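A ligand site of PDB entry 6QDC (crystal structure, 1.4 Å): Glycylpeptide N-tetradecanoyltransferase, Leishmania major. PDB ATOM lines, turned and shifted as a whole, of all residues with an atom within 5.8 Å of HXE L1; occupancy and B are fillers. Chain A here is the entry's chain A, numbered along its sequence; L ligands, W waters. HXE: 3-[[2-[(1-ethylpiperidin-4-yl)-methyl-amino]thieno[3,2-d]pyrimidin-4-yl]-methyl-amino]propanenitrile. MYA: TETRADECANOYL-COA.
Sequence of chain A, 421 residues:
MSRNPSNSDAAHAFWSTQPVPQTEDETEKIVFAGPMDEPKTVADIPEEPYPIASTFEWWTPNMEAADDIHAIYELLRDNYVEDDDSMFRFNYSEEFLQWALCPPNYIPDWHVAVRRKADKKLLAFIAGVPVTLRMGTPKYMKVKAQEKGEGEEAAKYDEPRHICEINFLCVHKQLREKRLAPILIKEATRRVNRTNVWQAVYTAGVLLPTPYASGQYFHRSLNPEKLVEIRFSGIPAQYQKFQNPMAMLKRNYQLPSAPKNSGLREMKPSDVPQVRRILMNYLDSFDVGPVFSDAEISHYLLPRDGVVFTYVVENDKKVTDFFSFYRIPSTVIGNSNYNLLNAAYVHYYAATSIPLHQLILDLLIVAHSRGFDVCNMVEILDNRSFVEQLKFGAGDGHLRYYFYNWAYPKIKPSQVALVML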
ATOM      1  N   TYR A  80      -7.285  23.882 -28.912  1.00  0.00           N
ATOM      2  CA  TYR A  80      -8.312  22.835 -28.749  1.00  0.00           C
ATOM      3  C   TYR A  80      -9.526  23.107 -29.634  1.00  0.00           C
ATOM      4  O   TYR A  80      -9.489  23.905 -30.566  1.00  0.00           O
ATOM      5  CB  TYR A  80      -8.634  22.598 -27.266  1.00  0.00           C
ATOM      6  CG  TYR A  80      -9.263  21.252 -26.920  1.00  0.00           C
ATOM      7  CD1 TYR A  80      -8.785  20.060 -27.436  1.00  0.00           C
ATOM      8  CD2 TYR A  80     -10.348  21.216 -26.038  1.00  0.00           C
ATOM      9  CE1 TYR A  80      -9.346  18.846 -27.052  1.00  0.00           C
ATOM     10  CE2 TYR A  80     -10.933  19.991 -25.669  1.00  0.00           C
ATOM     11  CZ  TYR A  80     -10.416  18.826 -26.165  1.00  0.00           C
ATOM     12  OH  TYR A  80     -11.009  17.651 -25.815  1.00  0.00           O
ATOM     13  N   VAL A  81     -10.631  22.378 -29.384  1.00  0.00           N
ATOM     14  CA  VAL A  81     -11.689  22.353 -30.399  1.00  0.00           C
ATOM     15  C   VAL A  81     -12.320  23.745 -30.585  1.00  0.00           C
ATOM     16  O   VAL A  81     -12.642  24.453 -29.626  1.00  0.00           O
ATOM     17  CB  VAL A  81     -12.830  21.369 -29.999  1.00  0.00           C
ATOM     18  CG1 VAL A  81     -13.722  21.125 -31.205  1.00  0.00           C
ATOM     19  CG2 VAL A  81     -12.342  20.006 -29.493  1.00  0.00           C
ATOM     20  N   PHE A  90     -12.950  26.203 -27.099  1.00  0.00           N
ATOM     21  CA  PHE A  90     -13.021  25.941 -25.661  1.00  0.00           C
ATOM     22  C   PHE A  90     -11.832  26.501 -24.895  1.00  0.00           C
ATOM     23  O   PHE A  90     -10.729  26.547 -25.392  1.00  0.00           O
ATOM     24  CB  PHE A  90     -13.044  24.425 -25.418  1.00  0.00           C
ATOM     25  CG  PHE A  90     -14.313  23.783 -25.919  1.00  0.00           C
ATOM     26  CD1 PHE A  90     -15.556  24.097 -25.339  1.00  0.00           C
ATOM     27  CD2 PHE A  90     -14.237  22.859 -26.978  1.00  0.00           C
ATOM     28  CE1 PHE A  90     -16.723  23.526 -25.847  1.00  0.00           C
ATOM     29  CE2 PHE A  90     -15.409  22.268 -27.450  1.00  0.00           C
ATOM     30  CZ  PHE A  90     -16.622  22.619 -26.920  1.00  0.00           C
ATOM     31  N   TYR A  92     -11.147  25.549 -21.349  1.00  0.00           N
ATOM     32  CA  TYR A  92     -11.193  24.813 -20.083  1.00  0.00           C
ATOM     33  C   TYR A  92     -10.223  25.435 -19.086  1.00  0.00           C
ATOM     34  O   TYR A  92      -9.070  25.694 -19.432  1.00  0.00           O
ATOM     35  CB  TYR A  92     -10.797  23.343 -20.322  1.00  0.00           C
ATOM     36  CG  TYR A  92     -11.801  22.426 -20.982  1.00  0.00           C
ATOM     37  CD1 TYR A  92     -11.909  22.330 -22.346  1.00  0.00           C
ATOM     38  CD2 TYR A  92     -12.650  21.620 -20.190  1.00  0.00           C
ATOM     39  CE1 TYR A  92     -12.824  21.469 -22.946  1.00  0.00           C
ATOM     40  CE2 TYR A  92     -13.522  20.726 -20.796  1.00  0.00           C
ATOM     41  CZ  TYR A  92     -13.585  20.644 -22.174  1.00  0.00           C
ATOM     42  OH  TYR A  92     -14.459  19.743 -22.751  1.00  0.00           O
ATOM     43  N   ILE A 166     -10.506   8.418 -22.488  1.00  0.00           N
ATOM     44  CA  ILE A 166      -9.608   9.362 -23.170  1.00  0.00           C
ATOM     45  C   ILE A 166     -10.274  10.704 -23.412  1.00  0.00           C
ATOM     46  O   ILE A 166     -11.442  10.737 -23.818  1.00  0.00           O
ATOM     47  CB  ILE A 166      -9.134   8.735 -24.503  1.00  0.00           C
ATOM     48  CG1 ILE A 166      -8.234   7.494 -24.315  1.00  0.00           C
ATOM     49  CG2 ILE A 166      -8.412   9.769 -25.419  1.00  0.00           C
ATOM     50  CD1 ILE A 166      -6.827   7.806 -23.808  1.00  0.00           C
ATOM     51  N   ASN A 167      -9.502  11.787 -23.249  1.00  0.00           N
ATOM     52  CA  ASN A 167     -10.020  13.138 -23.480  1.00  0.00           C
ATOM     53  C   ASN A 167      -8.845  14.052 -23.814  1.00  0.00           C
ATOM     54  O   ASN A 167      -7.693  13.671 -23.652  1.00  0.00           O
ATOM     55  CB  ASN A 167     -10.719  13.624 -22.185  1.00  0.00           C
ATOM     56  CG  ASN A 167     -11.797  14.672 -22.431  1.00  0.00           C
ATOM     57  OD1 ASN A 167     -11.830  15.367 -23.424  1.00  0.00           O
ATOM     58  ND2 ASN A 167     -12.763  14.726 -21.530  1.00  0.00           N
ATOM     59  N   PHE A 168      -9.156  15.267 -24.306  1.00  0.00           N
ATOM     60  CA  PHE A 168      -8.175  16.335 -24.456  1.00  0.00           C
ATOM     61  C   PHE A 168      -7.078  16.040 -25.474  1.00  0.00           C
ATOM     62  O   PHE A 168      -6.001  16.604 -25.365  1.00  0.00           O
ATOM     63  CB  PHE A 168      -7.629  16.746 -23.082  1.00  0.00           C
ATOM     64  CG  PHE A 168      -8.672  17.203 -22.123  1.00  0.00           C
ATOM     65  CD1 PHE A 168      -9.386  18.368 -22.381  1.00  0.00           C
ATOM     66  CD2 PHE A 168      -8.926  16.508 -20.960  1.00  0.00           C
ATOM     67  CE1 PHE A 168     -10.396  18.802 -21.530  1.00  0.00           C
ATOM     68  CE2 PHE A 168      -9.951  16.923 -20.104  1.00  0.00           C
ATOM     69  CZ  PHE A 168     -10.665  18.092 -20.372  1.00  0.00           C
ATOM     70  N   THR A 203     -15.101  10.046 -26.746  1.00  0.00           N
ATOM     71  CA  THR A 203     -16.163  10.718 -27.521  1.00  0.00           C
ATOM     72  C   THR A 203     -15.494  11.710 -28.461  1.00  0.00           C
ATOM     73  O   THR A 203     -14.363  12.163 -28.233  1.00  0.00           O
ATOM     74  CB  THR A 203     -17.197  11.407 -26.637  1.00  0.00           C
ATOM     75  OG1 THR A 203     -16.565  12.355 -25.751  1.00  0.00           O
ATOM     76  CG2 THR A 203     -18.035  10.412 -25.872  1.00  0.00           C
ATOM     77  N   ALA A 204     -16.195  12.087 -29.540  1.00  0.00           N
ATOM     78  CA  ALA A 204     -15.748  13.173 -30.407  1.00  0.00           C
ATOM     79  C   ALA A 204     -16.977  13.724 -31.119  1.00  0.00           C
ATOM     80  O   ALA A 204     -17.996  13.066 -31.259  1.00  0.00           O
ATOM     81  CB  ALA A 204     -14.752  12.659 -31.424  1.00  0.00           C
ATOM     82  N   GLY A 205     -16.871  14.981 -31.557  1.00  0.00           N
ATOM     83  CA  GLY A 205     -17.830  15.584 -32.458  1.00  0.00           C
ATOM     84  C   GLY A 205     -17.734  14.981 -33.857  1.00  0.00           C
ATOM     85  O   GLY A 205     -18.764  14.810 -34.556  1.00  0.00           O
ATOM     86  N   VAL A 206     -16.550  14.633 -34.326  1.00  0.00           N
ATOM     87  CA  VAL A 206     -16.361  14.142 -35.681  1.00  0.00           C
ATOM     88  C   VAL A 206     -16.749  12.673 -35.756  1.00  0.00           C
ATOM     89  O   VAL A 206     -16.736  11.941 -34.764  1.00  0.00           O
ATOM     90  CB  VAL A 206     -14.938  14.413 -36.185  1.00  0.00           C
ATOM     91  CG1 VAL A 206     -14.706  15.924 -36.263  1.00  0.00           C
ATOM     92  CG2 VAL A 206     -13.857  13.690 -35.360  1.00  0.00           C
ATOM     93  N   TYR A 217     -26.419  17.531 -29.504  1.00  0.00           N
ATOM     94  CA  TYR A 217     -26.356  18.549 -28.456  1.00  0.00           C
ATOM     95  C   TYR A 217     -27.606  19.399 -28.390  1.00  0.00           C
ATOM     96  O   TYR A 217     -28.255  19.623 -29.433  1.00  0.00           O
ATOM     97  CB  TYR A 217     -25.207  19.517 -28.767  1.00  0.00           C
ATOM     98  CG  TYR A 217     -23.923  19.022 -28.120  1.00  0.00           C
ATOM     99  CD1 TYR A 217     -23.682  19.341 -26.807  1.00  0.00           C
ATOM    100  CD2 TYR A 217     -23.008  18.229 -28.810  1.00  0.00           C
ATOM    101  CE1 TYR A 217     -22.524  18.840 -26.169  1.00  0.00           C
ATOM    102  CE2 TYR A 217     -21.853  17.754 -28.187  1.00  0.00           C
ATOM    103  CZ  TYR A 217     -21.607  18.054 -26.846  1.00  0.00           C
ATOM    104  OH  TYR A 217     -20.519  17.484 -26.199  1.00  0.00           O
ATOM    105  N   HIS A 219     -29.154  23.062 -26.332  1.00  0.00           N
ATOM    106  CA  HIS A 219     -28.786  24.310 -25.652  1.00  0.00           C
ATOM    107  C   HIS A 219     -30.036  24.942 -25.053  1.00  0.00           C
ATOM    108  O   HIS A 219     -31.090  24.872 -25.666  1.00  0.00           O
ATOM    109  CB  HIS A 219     -28.056  25.223 -26.641  1.00  0.00           C
ATOM    110  CG  HIS A 219     -27.099  24.480 -27.522  1.00  0.00           C
ATOM    111  ND1 HIS A 219     -25.927  23.997 -27.003  1.00  0.00           N
ATOM    112  CD2 HIS A 219     -27.160  24.019 -28.811  1.00  0.00           C
ATOM    113  CE1 HIS A 219     -25.288  23.305 -27.909  1.00  0.00           C
ATOM    114  NE2 HIS A 219     -26.017  23.277 -29.010  1.00  0.00           N
ATOM    115  N   PHE A 232     -23.737  32.932 -31.292  1.00  0.00           N
ATOM    116  CA  PHE A 232     -24.023  31.583 -30.846  1.00  0.00           C
ATOM    117  C   PHE A 232     -25.415  31.213 -31.315  1.00  0.00           C
ATOM    118  O   PHE A 232     -25.649  30.102 -31.684  1.00  0.00           O
ATOM    119  CB  PHE A 232     -23.967  31.515 -29.300  1.00  0.00           C
ATOM    120  CG  PHE A 232     -24.230  30.165 -28.676  1.00  0.00           C
ATOM    121  CD1 PHE A 232     -25.521  29.711 -28.459  1.00  0.00           C
ATOM    122  CD2 PHE A 232     -23.173  29.343 -28.332  1.00  0.00           C
ATOM    123  CE1 PHE A 232     -25.734  28.437 -27.928  1.00  0.00           C
ATOM    124  CE2 PHE A 232     -23.401  28.124 -27.715  1.00  0.00           C
ATOM    125  CZ  PHE A 232     -24.688  27.682 -27.505  1.00  0.00           C
ATOM    126  N   ILE A 328     -17.684  25.133 -18.556  1.00  0.00           N
ATOM    127  CA  ILE A 328     -16.599  25.176 -19.540  1.00  0.00           C
ATOM    128  C   ILE A 328     -16.805  26.485 -20.292  1.00  0.00           C
ATOM    129  O   ILE A 328     -17.749  26.638 -21.090  1.00  0.00           O
ATOM    130  CB  ILE A 328     -16.635  24.027 -20.568  1.00  0.00           C
ATOM    131  CG1 ILE A 328     -16.642  22.660 -19.863  1.00  0.00           C
ATOM    132  CG2 ILE A 328     -15.390  24.197 -21.470  1.00  0.00           C
ATOM    133  CD1 ILE A 328     -16.948  21.509 -20.845  1.00  0.00           C
ATOM    134  N   TYR A 345     -22.899  22.958 -18.174  1.00  0.00           N
ATOM    135  CA  TYR A 345     -23.213  21.678 -18.828  1.00  0.00           C
ATOM    136  C   TYR A 345     -23.885  20.787 -17.820  1.00  0.00           C
ATOM    137  O   TYR A 345     -23.449  20.650 -16.643  1.00  0.00           O
ATOM    138  CB  TYR A 345     -21.924  20.951 -19.232  1.00  0.00           C
ATOM    139  CG  TYR A 345     -21.331  21.489 -20.520  1.00  0.00           C
ATOM    140  CD1 TYR A 345     -20.685  22.729 -20.531  1.00  0.00           C
ATOM    141  CD2 TYR A 345     -21.441  20.802 -21.714  1.00  0.00           C
ATOM    142  CE1 TYR A 345     -20.169  23.244 -21.694  1.00  0.00           C
ATOM    143  CE2 TYR A 345     -20.921  21.334 -22.904  1.00  0.00           C
ATOM    144  CZ  TYR A 345     -20.289  22.555 -22.868  1.00  0.00           C
ATOM    145  OH  TYR A 345     -19.705  23.091 -24.022  1.00  0.00           O
ATOM    146  N   ASN A 376     -25.834  23.594 -21.675  1.00  0.00           N
ATOM    147  CA  ASN A 376     -25.659  22.615 -22.752  1.00  0.00           C
ATOM    148  C   ASN A 376     -25.816  21.203 -22.201  1.00  0.00           C
ATOM    149  O   ASN A 376     -25.521  20.963 -21.016  1.00  0.00           O
ATOM    150  CB  ASN A 376     -24.243  22.750 -23.343  1.00  0.00           C
ATOM    151  CG  ASN A 376     -24.049  24.077 -24.049  1.00  0.00           C
ATOM    152  OD1 ASN A 376     -24.918  24.541 -24.763  1.00  0.00           O
ATOM    153  ND2 ASN A 376     -22.888  24.680 -23.853  1.00  0.00           N
ATOM    154  N   GLY A 397     -24.665  20.244 -33.481  1.00  0.00           N
ATOM    155  CA  GLY A 397     -23.556  19.348 -33.195  1.00  0.00           C
ATOM    156  C   GLY A 397     -24.068  18.039 -32.626  1.00  0.00           C
ATOM    157  O   GLY A 397     -25.242  17.890 -32.191  1.00  0.00           O
ATOM    158  N   HIS A 398     -23.170  17.072 -32.659  1.00  0.00           N
ATOM    159  CA  HIS A 398     -23.445  15.794 -32.049  1.00  0.00           C
ATOM    160  C   HIS A 398     -22.245  15.397 -31.206  1.00  0.00           C
ATOM    161  O   HIS A 398     -21.098  15.925 -31.309  1.00  0.00           O
ATOM    162  CB  HIS A 398     -23.590  14.740 -33.121  1.00  0.00           C
ATOM    163  CG  HIS A 398     -24.659  15.017 -34.131  1.00  0.00           C
ATOM    164  ND1 HIS A 398     -25.908  14.421 -34.103  1.00  0.00           N
ATOM    165  CD2 HIS A 398     -24.677  15.887 -35.151  1.00  0.00           C
ATOM    166  CE1 HIS A 398     -26.635  14.889 -35.098  1.00  0.00           C
ATOM    167  NE2 HIS A 398     -25.883  15.790 -35.748  1.00  0.00           N
ATOM    168  N   LEU A 399     -22.505  14.501 -30.281  1.00  0.00           N
ATOM    169  CA  LEU A 399     -21.411  13.796 -29.616  1.00  0.00           C
ATOM    170  C   LEU A 399     -21.525  12.325 -29.966  1.00  0.00           C
ATOM    171  O   LEU A 399     -22.570  11.701 -29.686  1.00  0.00           O
ATOM    172  CB  LEU A 399     -21.440  14.030 -28.111  1.00  0.00           C
ATOM    173  CG  LEU A 399     -20.168  13.601 -27.376  1.00  0.00           C
ATOM    174  CD1 LEU A 399     -18.969  14.457 -27.837  1.00  0.00           C
ATOM    175  CD2 LEU A 399     -20.346  13.664 -25.881  1.00  0.00           C
ATOM    176  N   MET A 420     -19.338  12.853 -20.525  1.00  0.00           N
ATOM    177  CA  MET A 420     -17.943  13.087 -20.865  1.00  0.00           C
ATOM    178  C   MET A 420     -17.630  14.585 -20.818  1.00  0.00           C
ATOM    179  O   MET A 420     -18.371  15.396 -21.364  1.00  0.00           O
ATOM    180  CB  MET A 420     -17.719  12.573 -22.286  1.00  0.00           C
ATOM    181  CG  MET A 420     -17.948  11.080 -22.359  1.00  0.00           C
ATOM    182  SD  MET A 420     -16.589  10.280 -21.569  1.00  0.00           S
ATOM    183  CE  MET A 420     -15.594  10.171 -23.052  1.00  0.00           C
ATOM    184  N   LEU A 421     -16.566  14.915 -20.066  1.00  0.00           N
ATOM    185  CA  LEU A 421     -16.256  16.313 -19.806  1.00  0.00           C
ATOM    186  C   LEU A 421     -15.629  17.010 -21.000  1.00  0.00           C
ATOM    187  O   LEU A 421     -14.954  16.454 -21.891  1.00  0.00           O
ATOM    188  CB  LEU A 421     -15.287  16.348 -18.618  1.00  0.00           C
ATOM    189  CG  LEU A 421     -15.811  15.719 -17.340  1.00  0.00           C
ATOM    190  CD1 LEU A 421     -14.710  15.787 -16.291  1.00  0.00           C
ATOM    191  CD2 LEU A 421     -17.102  16.397 -16.834  1.00  0.00           C
ATOM    192  OXT LEU A 421     -15.861  18.230 -21.157  1.00  0.00           O
HETATM  193  N4  HXE L   1     -15.153  17.351 -30.178  1.00  0.00           N
HETATM  194  C13 HXE L   1     -16.046  18.146 -30.148  1.00  0.00           C
HETATM  195  C12 HXE L   1     -17.208  19.064 -30.225  1.00  0.00           C
HETATM  196  C11 HXE L   1     -18.672  18.501 -29.983  1.00  0.00           C
HETATM  197  N3  HXE L   1     -19.538  19.699 -29.849  1.00  0.00           N
HETATM  198  C10 HXE L   1     -20.400  20.170 -30.954  1.00  0.00           C
HETATM  199  C9  HXE L   1     -19.682  20.364 -28.633  1.00  0.00           C
HETATM  200  N2  HXE L   1     -18.805  19.844 -27.757  1.00  0.00           N
HETATM  201  C14 HXE L   1     -20.594  21.301 -28.278  1.00  0.00           C
HETATM  202  C17 HXE L   1     -20.575  21.799 -27.003  1.00  0.00           C
HETATM  203  C16 HXE L   1     -21.453  22.822 -26.646  1.00  0.00           C
HETATM  204  C15 HXE L   1     -22.265  23.136 -27.736  1.00  0.00           C
HETATM  205  S   HXE L   1     -21.843  22.241 -29.099  1.00  0.00           S
HETATM  206  N5  HXE L   1     -19.687  21.318 -26.086  1.00  0.00           N
HETATM  207  C8  HXE L   1     -18.854  20.320 -26.491  1.00  0.00           C
HETATM  208  N1  HXE L   1     -17.930  19.747 -25.626  1.00  0.00           N
HETATM  209  C7  HXE L   1     -17.760  20.341 -24.308  1.00  0.00           C
HETATM  210  C4  HXE L   1     -17.174  18.422 -25.933  1.00  0.00           C
HETATM  211  C3  HXE L   1     -17.323  17.608 -24.629  1.00  0.00           C
HETATM  212  C2  HXE L   1     -16.596  16.238 -24.660  1.00  0.00           C
HETATM  213  C5  HXE L   1     -15.676  18.724 -26.156  1.00  0.00           C
HETATM  214  C6  HXE L   1     -15.060  17.302 -26.475  1.00  0.00           C
HETATM  215  N   HXE L   1     -15.334  16.308 -25.410  1.00  0.00           N
HETATM  216  C1  HXE L   1     -14.570  15.029 -25.261  1.00  0.00           C
HETATM  217  C   HXE L   1     -13.565  14.933 -26.326  1.00  0.00           C
HETATM  218  S1  MYA L   2     -12.002  14.480 -29.415  1.00  0.00           S
HETATM  219  C2  MYA L   2     -11.270  16.154 -29.414  1.00  0.00           C
HETATM  220  C3  MYA L   2     -10.099  16.131 -30.400  1.00  0.00           C
HETATM  221  N4  MYA L   2      -9.393  17.437 -30.401  1.00  0.00           N
HETATM  222  C5  MYA L   2      -9.642  18.438 -31.234  1.00  0.00           C
HETATM  223  O5  MYA L   2     -10.547  18.392 -32.090  1.00  0.00           O
HETATM  224  C6  MYA L   2      -8.771  19.652 -31.022  1.00  0.00           C
HETATM  225  C7  MYA L   2      -8.435  20.394 -32.364  1.00  0.00           C
HETATM  226  N8  MYA L   2      -7.803  19.491 -33.356  1.00  0.00           N
HETATM  227  C9  MYA L   2      -6.670  18.921 -33.191  1.00  0.00           C
HETATM  228  O9  MYA L   2      -5.968  19.163 -32.182  1.00  0.00           O
HETATM  229  C10 MYA L   2      -6.158  17.999 -34.267  1.00  0.00           C
HETATM  230  O10 MYA L   2      -6.874  18.288 -35.441  1.00  0.00           O
HETATM  231  C11 MYA L   2      -6.292  16.486 -33.884  1.00  0.00           C
HETATM  232  C12 MYA L   2      -5.928  15.638 -35.042  1.00  0.00           C
HETATM  233  C13 MYA L   2      -7.720  16.128 -33.485  1.00  0.00           C
HETATM  234  C14 MYA L   2      -5.364  16.178 -32.693  1.00  0.00           C
HETATM  235  N1A MYA L   2     -10.042  11.483 -32.573  1.00  0.00           N
HETATM  236  O1A MYA L   2      -2.089  14.181 -36.806  1.00  0.00           O
HETATM  237  P1A MYA L   2      -2.976  14.028 -37.917  1.00  0.00           P
HETATM  238  C1X MYA L   2      -7.577  11.066 -37.031  1.00  0.00           C
HETATM  239  C2A MYA L   2      -9.378  10.444 -33.133  1.00  0.00           C
HETATM  240  O2A MYA L   2      -2.335  14.172 -39.261  1.00  0.00           O
HETATM  241  P2A MYA L   2      -4.335  16.425 -37.039  1.00  0.00           P
HETATM  242  C2M MYA L   2     -10.975  13.696 -28.268  1.00  0.00           C
HETATM  243  O2M MYA L   2     -10.196  14.314 -27.541  1.00  0.00           O
HETATM  244  C2X MYA L   2      -7.919  11.261 -38.519  1.00  0.00           C
HETATM  245  O2X MYA L   2      -9.071  10.544 -38.816  1.00  0.00           O
HETATM  246  N3A MYA L   2      -8.766  10.472 -34.333  1.00  0.00           N
HETATM  247  O3A MYA L   2      -4.234  15.044 -37.860  1.00  0.00           O
HETATM  248  C3M MYA L   2     -11.064  12.214 -28.165  1.00  0.00           C
HETATM  249  C3X MYA L   2      -6.649  10.667 -39.118  1.00  0.00           C
HETATM  250  O3X MYA L   2      -6.689   9.215 -39.097  1.00  0.00           O
HETATM  251  P3X MYA L   2      -7.078   8.387 -40.435  1.00  0.00           P
HETATM  252  C4A MYA L   2      -8.830  11.649 -35.018  1.00  0.00           C
HETATM  253  O4A MYA L   2      -5.486  17.136 -37.550  1.00  0.00           O
HETATM  254  C4M MYA L   2      -9.769  11.636 -28.810  1.00  0.00           C
HETATM  255  C4X MYA L   2      -5.528  11.083 -38.186  1.00  0.00           C
HETATM  256  O4X MYA L   2      -6.219  11.489 -36.963  1.00  0.00           O
HETATM  257  C5A MYA L   2      -9.511  12.705 -34.507  1.00  0.00           C
HETATM  258  O5A MYA L   2      -3.074  17.138 -36.995  1.00  0.00           O
HETATM  259  C5M MYA L   2      -9.862  10.114 -28.955  1.00  0.00           C
HETATM  260  C5X MYA L   2      -4.788  12.312 -38.690  1.00  0.00           C
HETATM  261  O5X MYA L   2      -3.738  12.662 -37.800  1.00  0.00           O
HETATM  262  C6A MYA L   2     -10.122  12.602 -33.264  1.00  0.00           C
HETATM  263  N6A MYA L   2     -10.842  13.626 -32.711  1.00  0.00           N
HETATM  264  O6A MYA L   2      -4.599  16.014 -35.484  1.00  0.00           O
HETATM  265  C6M MYA L   2      -8.550   9.556 -29.532  1.00  0.00           C
HETATM  266  N7A MYA L   2      -9.393  13.728 -35.438  1.00  0.00           N
HETATM  267  O7A MYA L   2      -8.440   8.890 -40.836  1.00  0.00           O
HETATM  268  C7M MYA L   2      -8.549   8.043 -29.763  1.00  0.00           C
HETATM  269  C8A MYA L   2      -8.653  13.261 -36.447  1.00  0.00           C
HETATM  270  O8A MYA L   2      -6.009   8.787 -41.381  1.00  0.00           O
HETATM  271  C8M MYA L   2      -8.400   7.296 -28.415  1.00  0.00           C
HETATM  272  N9A MYA L   2      -8.351  11.953 -36.196  1.00  0.00           N
HETATM  273  O9A MYA L   2      -7.112   6.939 -40.041  1.00  0.00           O
HETATM  274  C9M MYA L   2      -8.193   5.775 -28.668  1.00  0.00           C
HETATM  275  CAM MYA L   2      -7.978   4.970 -27.373  1.00  0.00           C
HETATM  276  CBM MYA L   2      -6.522   5.041 -26.935  1.00  0.00           C
HETATM  277  CCM MYA L   2      -6.258   4.263 -25.589  1.00  0.00           C
HETATM  278  CDM MYA L   2      -6.571   2.766 -25.719  1.00  0.00           C
HETATM  279  CEM MYA L   2      -6.229   2.082 -24.366  1.00  0.00           C
HETATM  280  CFM MYA L   2      -6.620   0.605 -24.454  1.00  0.00           C
HETATM  281  N4  HXE L   3     -20.851  26.546 -25.374  1.00  0.00           N
HETATM  282  C13 HXE L   3     -20.183  26.118 -26.253  1.00  0.00           C
HETATM  283  C12 HXE L   3     -19.303  25.515 -27.217  1.00  0.00           C
HETATM  284  C11 HXE L   3     -18.464  26.623 -27.891  1.00  0.00           C
HETATM  285  N3  HXE L   3     -17.758  25.880 -28.952  1.00  0.00           N
HETATM  286  C10 HXE L   3     -16.286  25.723 -28.798  1.00  0.00           C
HETATM  287  C9  HXE L   3     -18.403  25.395 -30.071  1.00  0.00           C
HETATM  288  N2  HXE L   3     -19.622  25.842 -30.292  1.00  0.00           N
HETATM  289  C14 HXE L   3     -17.896  24.368 -30.915  1.00  0.00           C
HETATM  290  C17 HXE L   3     -18.672  23.891 -31.968  1.00  0.00           C
HETATM  291  C16 HXE L   3     -18.101  22.867 -32.766  1.00  0.00           C
HETATM  292  C15 HXE L   3     -16.824  22.509 -32.343  1.00  0.00           C
HETATM  293  S   HXE L   3     -16.462  23.503 -30.913  1.00  0.00           S
HETATM  294  N5  HXE L   3     -19.883  24.407 -32.212  1.00  0.00           N
HETATM  295  C8  HXE L   3     -20.356  25.369 -31.362  1.00  0.00           C
HETATM  296  N1  HXE L   3     -21.605  25.973 -31.576  1.00  0.00           N
HETATM  297  C7  HXE L   3     -22.155  26.711 -30.457  1.00  0.00           C
HETATM  298  C4  HXE L   3     -22.252  25.912 -32.918  1.00  0.00           C
HETATM  299  C3  HXE L   3     -21.703  27.069 -33.751  1.00  0.00           C
HETATM  300  C2  HXE L   3     -22.296  26.904 -35.158  1.00  0.00           C
HETATM  301  C5  HXE L   3     -23.793  25.992 -32.796  1.00  0.00           C
HETATM  302  C6  HXE L   3     -24.385  27.108 -33.670  1.00  0.00           C
HETATM  303  N   HXE L   3     -23.743  27.101 -35.011  1.00  0.00           N
HETATM  304  C1  HXE L   3     -24.587  27.304 -36.214  1.00  0.00           C
HETATM  305  C   HXE L   3     -24.047  26.764 -37.542  1.00  0.00           C
HETATM  306  O   HOH W   1     -18.659  18.095 -21.581  1.00  0.00           O
HETATM  307  O   HOH W   2     -16.058  18.694 -33.357  1.00  0.00           O
HETATM  308  O   HOH W   3     -14.466  16.280 -32.821  1.00  0.00           O
HETATM  309  O   HOH W   4     -13.068  17.684 -24.120  1.00  0.00           O
HETATM  310  O   HOH W   5     -13.387  11.812 -25.107  1.00  0.00           O
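OH of Tyr 345 is in hydrogen-bond range of N5 of HXE L1 (2.7 Å).
A nitrogen (N) of HXE L1 lies within salt-bridge range of the chain-end carboxylate (O) of Leu 421, 3.5 Å away.
N of Gly 205 lies within hydrogen-bond range of N4 of HXE L1 (3.2 Å).
A nitrogen (N2) of HXE L1 sits close to the side-chain hydroxyl (OH) of Tyr 217, 3.3 Å away.
The side-chain amide nitrogen (ND2) of Asn 376 lies within hydrogen-bond range of a nitrogen (N4) of HXE L3 (3.2 Å).
Water W3 lies within hydrogen-bond range of N4 of HXE L1 (2.9 Å), N of Gly 205 (3.0 Å) and N of Val 206 (3.1 Å).
Water W4 lies within hydrogen-bond range of the side-chain hydroxyl (OH) of Tyr 80 (2.7 Å), the side-chain amide oxygen (OD1) of Asn 167 (2.7 Å), the side-chain hydroxyl (OH) of Tyr 92 (2.8 Å) and the chain-end carboxylate (O) of Leu 421 (3.2 Å).
Water W5 bridges O of Ile 166 and N of Thr 203.
Water W1 lies within hydrogen-bond range of the backbone carbonyl oxygen of Met 420 (2.7 Å) and the chain-end carboxylate of Leu 421 (2.8 Å).
A ring nitrogen (ND1) of His 219 is in hydrogen-bond range of the side-chain amide oxygen (OD1) of Asn 376.
The chain-end carboxylate (O) of Leu 421 is in hydrogen-bond range of the side-chain amide nitrogen (ND2) of Asn 167, 2.8 Å away.
OH of Tyr 92 sits at hydrogen-bond distance from OXT of Leu 421, 2.6 Å away.
N of Phe 90 lies within hydrogen-bond range of O of Val 81.
The backbone carbonyl oxygen (O) of Gly 397 is in hydrogen-bond range of the backbone NH (N) of Tyr 217, at 3.0 Å.
The side-chain amide oxygen of Asn 167 is in hydrogen-bond range of the side-chain hydroxyl of Tyr 80 (3.4 Å).
N of Phe 168 lies within hydrogen-bond range of OH of Tyr 80, at 3.4 Å.
Residues that only touch HXE L1: Tyr 80 (3.8 Å), Val 81 (3.9 Å), Phe 90 (3.2 Å), Tyr 92 (3.7 Å), Asn 167 (3.3 Å), Thr 203 (3.4 Å), His 219 (3.0 Å), Ile 328 (3.7 Å), Asn 376 (3.6 Å), Gly 397 (3.96 Å), His 398 (3.8 Å) and Met 420 (3.8 Å).
Within 4 Å of HXE L1: Tyr 80, Val 81, Phe 90, Tyr 92, Asn 167, Thr 203, Gly 205, Tyr 217, His 219, Ile 328, Tyr 345, Asn 376, Gly 397, His 398, Met 420 and Leu 421.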
